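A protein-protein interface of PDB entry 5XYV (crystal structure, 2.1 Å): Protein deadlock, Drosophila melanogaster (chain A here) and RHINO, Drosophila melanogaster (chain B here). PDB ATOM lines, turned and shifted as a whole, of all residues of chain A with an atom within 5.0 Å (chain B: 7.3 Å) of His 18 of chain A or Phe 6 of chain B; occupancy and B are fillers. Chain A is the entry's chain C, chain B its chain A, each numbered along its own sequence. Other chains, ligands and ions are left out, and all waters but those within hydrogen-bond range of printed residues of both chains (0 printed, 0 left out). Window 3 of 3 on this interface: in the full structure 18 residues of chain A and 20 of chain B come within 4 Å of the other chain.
The backbone carbonyl oxygen (O) of Ile 39 of chain B is in hydrogen-bond range of the side-chain sulfur (SG) of Cys 15 of chain A (3.3 Å). The backbone NH (N) of Ala 41 of chain B sits at hydrogen-bond distance from a ring nitrogen (ND1) of His 18 of chain A, at 3.1 Å.
N of Gly 7 of chain B lies within hydrogen-bond range of OD2 of Asp 40 of chain B (2.8 Å). The guanidinium group of Arg 10 of chain B is in salt-bridge range of the side-chain carboxylate of Asp 40 of chain B (2.7 Å). The indole nitrogen (NE1) of Trp 33 of chain B is in hydrogen-bond range of the side-chain carboxylate (OD2) of Asp 40 of chain B (2.9 Å). The backbone carbonyl oxygen of His 18 of chain A lies within hydrogen-bond range of the side-chain hydroxyl of Thr 22 of chain A (2.9 Å).
Among the printed residues, merely in contact across the chains: Cys 15 of chain A with Phe 30 of chain B (3.7 Å), Cys 15 of chain A with Ala 41 of chain B (3.3 Å), His 18 of chain A with Phe 6 of chain B (3.4 Å), His 18 of chain A with Ile 39 of chain B (3.9 Å), His 18 of chain A with Asp 40 of chain B (3.3 Å), Ile 19 of chain A with Phe 28 of chain B (3.8 Å), Ile 19 of chain A with Ala 41 of chain B (3.8 Å) and Thr 22 of chain A with Phe 28 of chain B (3.9 Å).
Of the printed residues of chain B, Cys 15 of chain A touches Phe 30, Ile 39 and Ala 41. Gln 17 of chain A touches none of the printed residues of chain B. His 18 of chain A touches four residues of chain B. Thr 21 of chain A touches none of the printed residues of chain B. Of the printed residues of chain A, Phe 6 of chain B touches His 18 (3.4 Å). Of the printed residues of chain A, Phe 28 of chain B touches Ile 19 (3.8 Å) and Thr 22 (3.9 Å). Printed residues of chain A within 4 Å of Phe 30 of chain B: Cys 15. Of the printed residues of chain A, Ile 39 of chain B touches Cys 15 (3.3 Å) and His 18 (3.9 Å). Of the printed residues of chain A, Ala 41 of chain B touches Cys 15 (3.3 Å), His 18 (3.1 Å) and Ile 19 (3.8 Å). The nearest residue of chain B that does not touch His 18 of chain A is Phe 28 of chain B (5.0 Å). The nearest printed residue of chain A that does not touch Phe 6 of chain B is Thr 21 of chain A (4.004 Å).
Of the 9 printed residues of chain A, 4 touch a printed residue of chain B. Hydrophobic or aromatic side chains of chain A that line the printed part of chain B: His 18 and Ile 19. Of the 16 printed residues of chain B, 6 touch a printed residue of chain A. Hydrophobic or aromatic side chains of chain B within 4 Å of the printed part of chain A: Phe 6, Phe 28, Phe 30, Ile 39 and Ala 41. Along chain B the printed residues that touch a printed residue of chain A span positions 6 to 41. Among the printed residues, 10 pairs touch across the chains. Among the printed residues, no Asp or Glu carboxylate lies within 4 Å of a Lys or Arg side-chain nitrogen of the other chain.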
ATOM      1  N   SER A  14       1.513  10.147 -14.158  1.00  0.00           N
ATOM      2  CA  SER A  14       1.349   9.917 -15.585  1.00  0.00           C
ATOM      3  C   SER A  14       0.768   8.534 -15.849  1.00  0.00           C
ATOM      4  O   SER A  14      -0.161   8.371 -16.655  1.00  0.00           O
ATOM      5  CB  SER A  14       2.691  10.069 -16.302  1.00  0.00           C
ATOM      6  OG  SER A  14       3.172  11.383 -16.142  1.00  0.00           O
ATOM      7  N   CYS A  15       1.305   7.545 -15.150  1.00  0.00           N
ATOM      8  CA  CYS A  15       0.786   6.191 -15.225  1.00  0.00           C
ATOM      9  C   CYS A  15      -0.659   6.130 -14.748  1.00  0.00           C
ATOM     10  O   CYS A  15      -1.457   5.403 -15.319  1.00  0.00           O
ATOM     11  CB  CYS A  15       1.651   5.212 -14.408  1.00  0.00           C
ATOM     12  SG  CYS A  15       3.273   4.890 -15.102  1.00  0.00           S
ATOM     13  N   TRP A  16      -0.996   6.915 -13.726  1.00  0.00           N
ATOM     14  CA  TRP A  16      -2.381   6.975 -13.275  1.00  0.00           C
ATOM     15  C   TRP A  16      -3.242   7.521 -14.385  1.00  0.00           C
ATOM     16  O   TRP A  16      -4.320   7.012 -14.655  1.00  0.00           O
ATOM     17  CB  TRP A  16      -2.540   7.838 -12.014  1.00  0.00           C
ATOM     18  CG  TRP A  16      -3.958   7.880 -11.489  1.00  0.00           C
ATOM     19  CD1 TRP A  16      -4.790   8.971 -11.423  1.00  0.00           C
ATOM     20  CD2 TRP A  16      -4.709   6.776 -10.959  1.00  0.00           C
ATOM     21  NE1 TRP A  16      -6.007   8.610 -10.878  1.00  0.00           N
ATOM     22  CE2 TRP A  16      -5.983   7.266 -10.589  1.00  0.00           C
ATOM     23  CE3 TRP A  16      -4.432   5.415 -10.764  1.00  0.00           C
ATOM     24  CZ2 TRP A  16      -6.966   6.445 -10.028  1.00  0.00           C
ATOM     25  CZ3 TRP A  16      -5.416   4.605 -10.215  1.00  0.00           C
ATOM     26  CH2 TRP A  16      -6.660   5.121  -9.851  1.00  0.00           C
ATOM     27  N   GLN A  17      -2.743   8.555 -15.048  1.00  0.00           N
ATOM     28  CA  GLN A  17      -3.498   9.191 -16.113  1.00  0.00           C
ATOM     29  C   GLN A  17      -3.723   8.198 -17.266  1.00  0.00           C
ATOM     30  O   GLN A  17      -4.764   8.228 -17.933  1.00  0.00           O
ATOM     31  CB  GLN A  17      -2.764  10.447 -16.585  1.00  0.00           C
ATOM     32  CG  GLN A  17      -3.640  11.502 -17.190  1.00  0.00           C
ATOM     33  CD  GLN A  17      -4.725  11.977 -16.230  1.00  0.00           C
ATOM     34  OE1 GLN A  17      -4.493  12.145 -15.025  1.00  0.00           O
ATOM     35  NE2 GLN A  17      -5.928  12.159 -16.756  1.00  0.00           N
ATOM     36  N   HIS A  18      -2.745   7.315 -17.473  1.00  0.00           N
ATOM     37  CA  HIS A  18      -2.868   6.209 -18.435  1.00  0.00           C
ATOM     38  C   HIS A  18      -4.015   5.272 -18.078  1.00  0.00           C
ATOM     39  O   HIS A  18      -4.803   4.884 -18.944  1.00  0.00           O
ATOM     40  CB  HIS A  18      -1.568   5.386 -18.509  1.00  0.00           C
ATOM     41  CG  HIS A  18      -0.417   6.122 -19.108  1.00  0.00           C
ATOM     42  ND1 HIS A  18       0.895   5.727 -18.928  1.00  0.00           N
ATOM     43  CD2 HIS A  18      -0.373   7.220 -19.902  1.00  0.00           C
ATOM     44  CE1 HIS A  18       1.692   6.554 -19.577  1.00  0.00           C
ATOM     45  NE2 HIS A  18       0.949   7.467 -20.176  1.00  0.00           N
ATOM     46  N   ILE A  19      -4.071   4.873 -16.811  1.00  0.00           N
ATOM     47  CA  ILE A  19      -5.169   4.040 -16.335  1.00  0.00           C
ATOM     48  C   ILE A  19      -6.518   4.751 -16.545  1.00  0.00           C
ATOM     49  O   ILE A  19      -7.464   4.149 -17.041  1.00  0.00           O
ATOM     50  CB  ILE A  19      -4.993   3.663 -14.852  1.00  0.00           C
ATOM     51  CG1 ILE A  19      -3.775   2.758 -14.680  1.00  0.00           C
ATOM     52  CG2 ILE A  19      -6.257   2.993 -14.296  1.00  0.00           C
ATOM     53  CD1 ILE A  19      -3.418   2.531 -13.258  1.00  0.00           C
ATOM     54  N   LEU A  20      -6.592   6.029 -16.196  1.00  0.00           N
ATOM     55  CA  LEU A  20      -7.816   6.794 -16.418  1.00  0.00           C
ATOM     56  C   LEU A  20      -8.186   6.894 -17.900  1.00  0.00           C
ATOM     57  O   LEU A  20      -9.329   6.735 -18.256  1.00  0.00           O
ATOM     58  CB  LEU A  20      -7.696   8.199 -15.816  1.00  0.00           C
ATOM     59  CG  LEU A  20      -7.489   8.251 -14.294  1.00  0.00           C
ATOM     60  CD1 LEU A  20      -7.259   9.689 -13.816  1.00  0.00           C
ATOM     61  CD2 LEU A  20      -8.667   7.644 -13.589  1.00  0.00           C
ATOM     62  N   THR A  21      -7.225   7.140 -18.776  1.00  0.00           N
ATOM     63  CA  THR A  21      -7.519   7.243 -20.204  1.00  0.00           C
ATOM     64  C   THR A  21      -8.083   5.942 -20.783  1.00  0.00           C
ATOM     65  O   THR A  21      -8.881   5.947 -21.726  1.00  0.00           O
ATOM     66  CB  THR A  21      -6.253   7.642 -20.975  1.00  0.00           C
ATOM     67  OG1 THR A  21      -5.833   8.931 -20.517  1.00  0.00           O
ATOM     68  CG2 THR A  21      -6.502   7.673 -22.490  1.00  0.00           C
ATOM     69  N   THR A  22      -7.665   4.833 -20.182  1.00  0.00           N
ATOM     70  CA  THR A  22      -8.021   3.488 -20.611  1.00  0.00           C
ATOM     71  C   THR A  22      -9.420   2.978 -20.170  1.00  0.00           C
ATOM     72  O   THR A  22     -10.116   2.316 -20.961  1.00  0.00           O
ATOM     73  CB  THR A  22      -6.928   2.513 -20.111  1.00  0.00           C
ATOM     74  OG1 THR A  22      -5.692   2.861 -20.746  1.00  0.00           O
ATOM     75  CG2 THR A  22      -7.270   1.060 -20.422  1.00  0.00           C
ATOM     76  N   PRO B   5       0.797  10.046 -27.051  1.00  0.00           N
ATOM     77  CA  PRO B   5       0.938   8.668 -27.553  1.00  0.00           C
ATOM     78  C   PRO B   5       1.720   7.775 -26.589  1.00  0.00           C
ATOM     79  O   PRO B   5       2.905   7.984 -26.365  1.00  0.00           O
ATOM     80  CB  PRO B   5       1.700   8.841 -28.879  1.00  0.00           C
ATOM     81  CG  PRO B   5       1.659  10.292 -29.181  1.00  0.00           C
ATOM     82  CD  PRO B   5       1.569  10.996 -27.866  1.00  0.00           C
ATOM     83  N   PHE B   6       1.042   6.803 -26.002  1.00  0.00           N
ATOM     84  CA  PHE B   6       1.683   5.966 -24.992  1.00  0.00           C
ATOM     85  C   PHE B   6       1.309   4.473 -25.139  1.00  0.00           C
ATOM     86  O   PHE B   6       0.432   4.120 -25.928  1.00  0.00           O
ATOM     87  CB  PHE B   6       1.333   6.487 -23.593  1.00  0.00           C
ATOM     88  CG  PHE B   6      -0.125   6.363 -23.239  1.00  0.00           C
ATOM     89  CD1 PHE B   6      -0.600   5.228 -22.600  1.00  0.00           C
ATOM     90  CD2 PHE B   6      -1.012   7.386 -23.521  1.00  0.00           C
ATOM     91  CE1 PHE B   6      -1.934   5.097 -22.259  1.00  0.00           C
ATOM     92  CE2 PHE B   6      -2.361   7.269 -23.177  1.00  0.00           C
ATOM     93  CZ  PHE B   6      -2.817   6.108 -22.548  1.00  0.00           C
ATOM     94  N   GLY B   7       1.994   3.599 -24.396  1.00  0.00           N
ATOM     95  CA  GLY B   7       1.705   2.177 -24.459  1.00  0.00           C
ATOM     96  C   GLY B   7       2.129   1.526 -25.766  1.00  0.00           C
ATOM     97  O   GLY B   7       3.147   1.912 -26.371  1.00  0.00           O
ATOM     98  N   VAL B   8       1.349   0.546 -26.217  1.00  0.00           N
ATOM     99  CA  VAL B   8       1.698  -0.177 -27.435  1.00  0.00           C
ATOM    100  C   VAL B   8       1.673   0.768 -28.627  1.00  0.00           C
ATOM    101  O   VAL B   8       2.393   0.564 -29.600  1.00  0.00           O
ATOM    102  CB  VAL B   8       0.756  -1.363 -27.697  1.00  0.00           C
ATOM    103  CG1 VAL B   8       1.081  -2.523 -26.748  1.00  0.00           C
ATOM    104  CG2 VAL B   8      -0.675  -0.929 -27.528  1.00  0.00           C
ATOM    105  N   ASN B   9       0.865   1.819 -28.512  1.00  0.00           N
ATOM    106  CA  ASN B   9       0.761   2.848 -29.537  1.00  0.00           C
ATOM    107  C   ASN B   9       2.062   3.603 -29.803  1.00  0.00           C
ATOM    108  O   ASN B   9       2.143   4.341 -30.776  1.00  0.00           O
ATOM    109  CB  ASN B   9      -0.317   3.871 -29.162  1.00  0.00           C
ATOM    110  CG  ASN B   9      -1.714   3.350 -29.370  1.00  0.00           C
ATOM    111  OD1 ASN B   9      -1.930   2.402 -30.132  1.00  0.00           O
ATOM    112  ND2 ASN B   9      -2.684   3.977 -28.695  1.00  0.00           N
ATOM    113  N   ARG B  10       3.070   3.459 -28.948  1.00  0.00           N
ATOM    114  CA  ARG B  10       4.348   4.097 -29.232  1.00  0.00           C
ATOM    115  C   ARG B  10       5.052   3.377 -30.368  1.00  0.00           C
ATOM    116  O   ARG B  10       5.958   3.937 -30.985  1.00  0.00           O
ATOM    117  CB  ARG B  10       5.268   4.118 -28.009  1.00  0.00           C
ATOM    118  CG  ARG B  10       4.815   4.975 -26.845  1.00  0.00           C
ATOM    119  CD  ARG B  10       5.956   5.038 -25.853  1.00  0.00           C
ATOM    120  NE  ARG B  10       5.588   5.609 -24.566  1.00  0.00           N
ATOM    121  CZ  ARG B  10       5.718   6.900 -24.250  1.00  0.00           C
ATOM    122  NH1 ARG B  10       6.197   7.754 -25.141  1.00  0.00           N
ATOM    123  NH2 ARG B  10       5.372   7.337 -23.042  1.00  0.00           N
ATOM    124  N   GLY B  11       4.634   2.134 -30.626  1.00  0.00           N
ATOM    125  CA  GLY B  11       5.254   1.285 -31.627  1.00  0.00           C
ATOM    126  C   GLY B  11       6.703   0.944 -31.323  1.00  0.00           C
ATOM    127  O   GLY B  11       7.524   0.853 -32.236  1.00  0.00           O
ATOM    128  N   PHE B  28      -3.027  -3.774 -14.505  1.00  0.00           N
ATOM    129  CA  PHE B  28      -2.151  -2.929 -15.312  1.00  0.00           C
ATOM    130  C   PHE B  28      -0.712  -3.234 -14.995  1.00  0.00           C
ATOM    131  O   PHE B  28      -0.334  -3.314 -13.824  1.00  0.00           O
ATOM    132  CB  PHE B  28      -2.420  -1.434 -15.075  1.00  0.00           C
ATOM    133  CG  PHE B  28      -3.709  -0.949 -15.687  1.00  0.00           C
ATOM    134  CD1 PHE B  28      -3.716  -0.343 -16.940  1.00  0.00           C
ATOM    135  CD2 PHE B  28      -4.919  -1.114 -15.023  1.00  0.00           C
ATOM    136  CE1 PHE B  28      -4.902   0.091 -17.511  1.00  0.00           C
ATOM    137  CE2 PHE B  28      -6.105  -0.682 -15.600  1.00  0.00           C
ATOM    138  CZ  PHE B  28      -6.092  -0.088 -16.847  1.00  0.00           C
ATOM    139  N   PHE B  30       3.142  -1.774 -15.433  1.00  0.00           N
ATOM    140  CA  PHE B  30       3.909  -0.564 -15.631  1.00  0.00           C
ATOM    141  C   PHE B  30       5.236  -0.960 -16.256  1.00  0.00           C
ATOM    142  O   PHE B  30       6.005  -1.718 -15.657  1.00  0.00           O
ATOM    143  CB  PHE B  30       4.075   0.179 -14.301  1.00  0.00           C
ATOM    144  CG  PHE B  30       2.758   0.464 -13.634  1.00  0.00           C
ATOM    145  CD1 PHE B  30       1.937   1.477 -14.108  1.00  0.00           C
ATOM    146  CD2 PHE B  30       2.308  -0.328 -12.582  1.00  0.00           C
ATOM    147  CE1 PHE B  30       0.698   1.730 -13.530  1.00  0.00           C
ATOM    148  CE2 PHE B  30       1.077  -0.078 -11.986  1.00  0.00           C
ATOM    149  CZ  PHE B  30       0.268   0.956 -12.467  1.00  0.00           C
ATOM    150  N   TRP B  33       9.924   0.919 -22.534  1.00  0.00           N
ATOM    151  CA  TRP B  33      10.118   0.504 -23.908  1.00  0.00           C
ATOM    152  C   TRP B  33      11.570   0.715 -24.377  1.00  0.00           C
ATOM    153  O   TRP B  33      12.293   1.577 -23.865  1.00  0.00           O
ATOM    154  CB  TRP B  33       9.155   1.256 -24.825  1.00  0.00           C
ATOM    155  CG  TRP B  33       7.722   1.229 -24.355  1.00  0.00           C
ATOM    156  CD1 TRP B  33       7.084   2.192 -23.623  1.00  0.00           C
ATOM    157  CD2 TRP B  33       6.757   0.183 -24.583  1.00  0.00           C
ATOM    158  NE1 TRP B  33       5.778   1.806 -23.384  1.00  0.00           N
ATOM    159  CE2 TRP B  33       5.555   0.583 -23.962  1.00  0.00           C
ATOM    160  CE3 TRP B  33       6.796  -1.049 -25.251  1.00  0.00           C
ATOM    161  CZ2 TRP B  33       4.394  -0.203 -24.000  1.00  0.00           C
ATOM    162  CZ3 TRP B  33       5.652  -1.822 -25.286  1.00  0.00           C
ATOM    163  CH2 TRP B  33       4.464  -1.397 -24.665  1.00  0.00           C
ATOM    164  N   SER B  38      10.409   6.625 -20.658  1.00  0.00           N
ATOM    165  CA  SER B  38       9.132   6.778 -19.959  1.00  0.00           C
ATOM    166  C   SER B  38       8.589   5.466 -19.402  1.00  0.00           C
ATOM    167  O   SER B  38       8.896   4.387 -19.901  1.00  0.00           O
ATOM    168  CB  SER B  38       8.101   7.402 -20.892  1.00  0.00           C
ATOM    169  OG  SER B  38       8.523   8.684 -21.317  1.00  0.00           O
ATOM    170  N   ILE B  39       7.773   5.571 -18.364  1.00  0.00           N
ATOM    171  CA  ILE B  39       7.093   4.421 -17.783  1.00  0.00           C
ATOM    172  C   ILE B  39       5.606   4.517 -18.098  1.00  0.00           C
ATOM    173  O   ILE B  39       4.992   5.543 -17.829  1.00  0.00           O
ATOM    174  CB  ILE B  39       7.337   4.350 -16.256  1.00  0.00           C
ATOM    175  CG1 ILE B  39       8.841   4.400 -15.989  1.00  0.00           C
ATOM    176  CG2 ILE B  39       6.713   3.086 -15.647  1.00  0.00           C
ATOM    177  CD1 ILE B  39       9.242   4.201 -14.539  1.00  0.00           C
ATOM    178  N   ASP B  40       5.039   3.465 -18.690  1.00  0.00           N
ATOM    179  CA  ASP B  40       3.643   3.488 -19.139  1.00  0.00           C
ATOM    180  C   ASP B  40       2.775   2.490 -18.358  1.00  0.00           C
ATOM    181  O   ASP B  40       3.204   1.373 -18.083  1.00  0.00           O
ATOM    182  CB  ASP B  40       3.545   3.181 -20.646  1.00  0.00           C
ATOM    183  CG  ASP B  40       4.100   4.306 -21.539  1.00  0.00           C
ATOM    184  OD1 ASP B  40       4.445   5.400 -21.057  1.00  0.00           O
ATOM    185  OD2 ASP B  40       4.171   4.107 -22.764  1.00  0.00           O
ATOM    186  N   ALA B  41       1.559   2.890 -17.985  1.00  0.00           N
ATOM    187  CA  ALA B  41       0.572   1.912 -17.532  1.00  0.00           C
ATOM    188  C   ALA B  41       0.007   1.209 -18.761  1.00  0.00           C
ATOM    189  O   ALA B  41      -0.428   1.860 -19.699  1.00  0.00           O
ATOM    190  CB  ALA B  41      -0.552   2.566 -16.718  1.00  0.00           C
ATOM    191  N   VAL B  42       0.066  -0.117 -18.779  1.00  0.00           N
ATOM    192  CA  VAL B  42      -0.519  -0.870 -19.878  1.00  0.00           C
ATOM    193  C   VAL B  42      -1.390  -1.977 -19.322  1.00  0.00           C
ATOM    194  O   VAL B  42      -0.961  -2.722 -18.454  1.00  0.00           O
ATOM    195  CB  VAL B  42       0.537  -1.483 -20.799  1.00  0.00           C
ATOM    196  CG1 VAL B  42      -0.132  -2.342 -21.845  1.00  0.00           C
ATOM    197  CG2 VAL B  42       1.345  -0.405 -21.473  1.00  0.00           C
ATOM    198  N   ASP B  46      -3.330  -5.813 -23.295  1.00  0.00           N
ATOM    199  CA  ASP B  46      -2.614  -5.222 -24.423  1.00  0.00           C
ATOM    200  C   ASP B  46      -1.260  -5.864 -24.710  1.00  0.00           C
ATOM    201  O   ASP B  46      -0.734  -5.705 -25.798  1.00  0.00           O
ATOM    202  CB  ASP B  46      -2.416  -3.717 -24.219  1.00  0.00           C
ATOM    203  CG  ASP B  46      -3.720  -2.957 -24.259  1.00  0.00           C
ATOM    204  OD1 ASP B  46      -4.737  -3.566 -24.673  1.00  0.00           O
ATOM    205  OD2 ASP B  46      -3.721  -1.752 -23.903  1.00  0.00           O
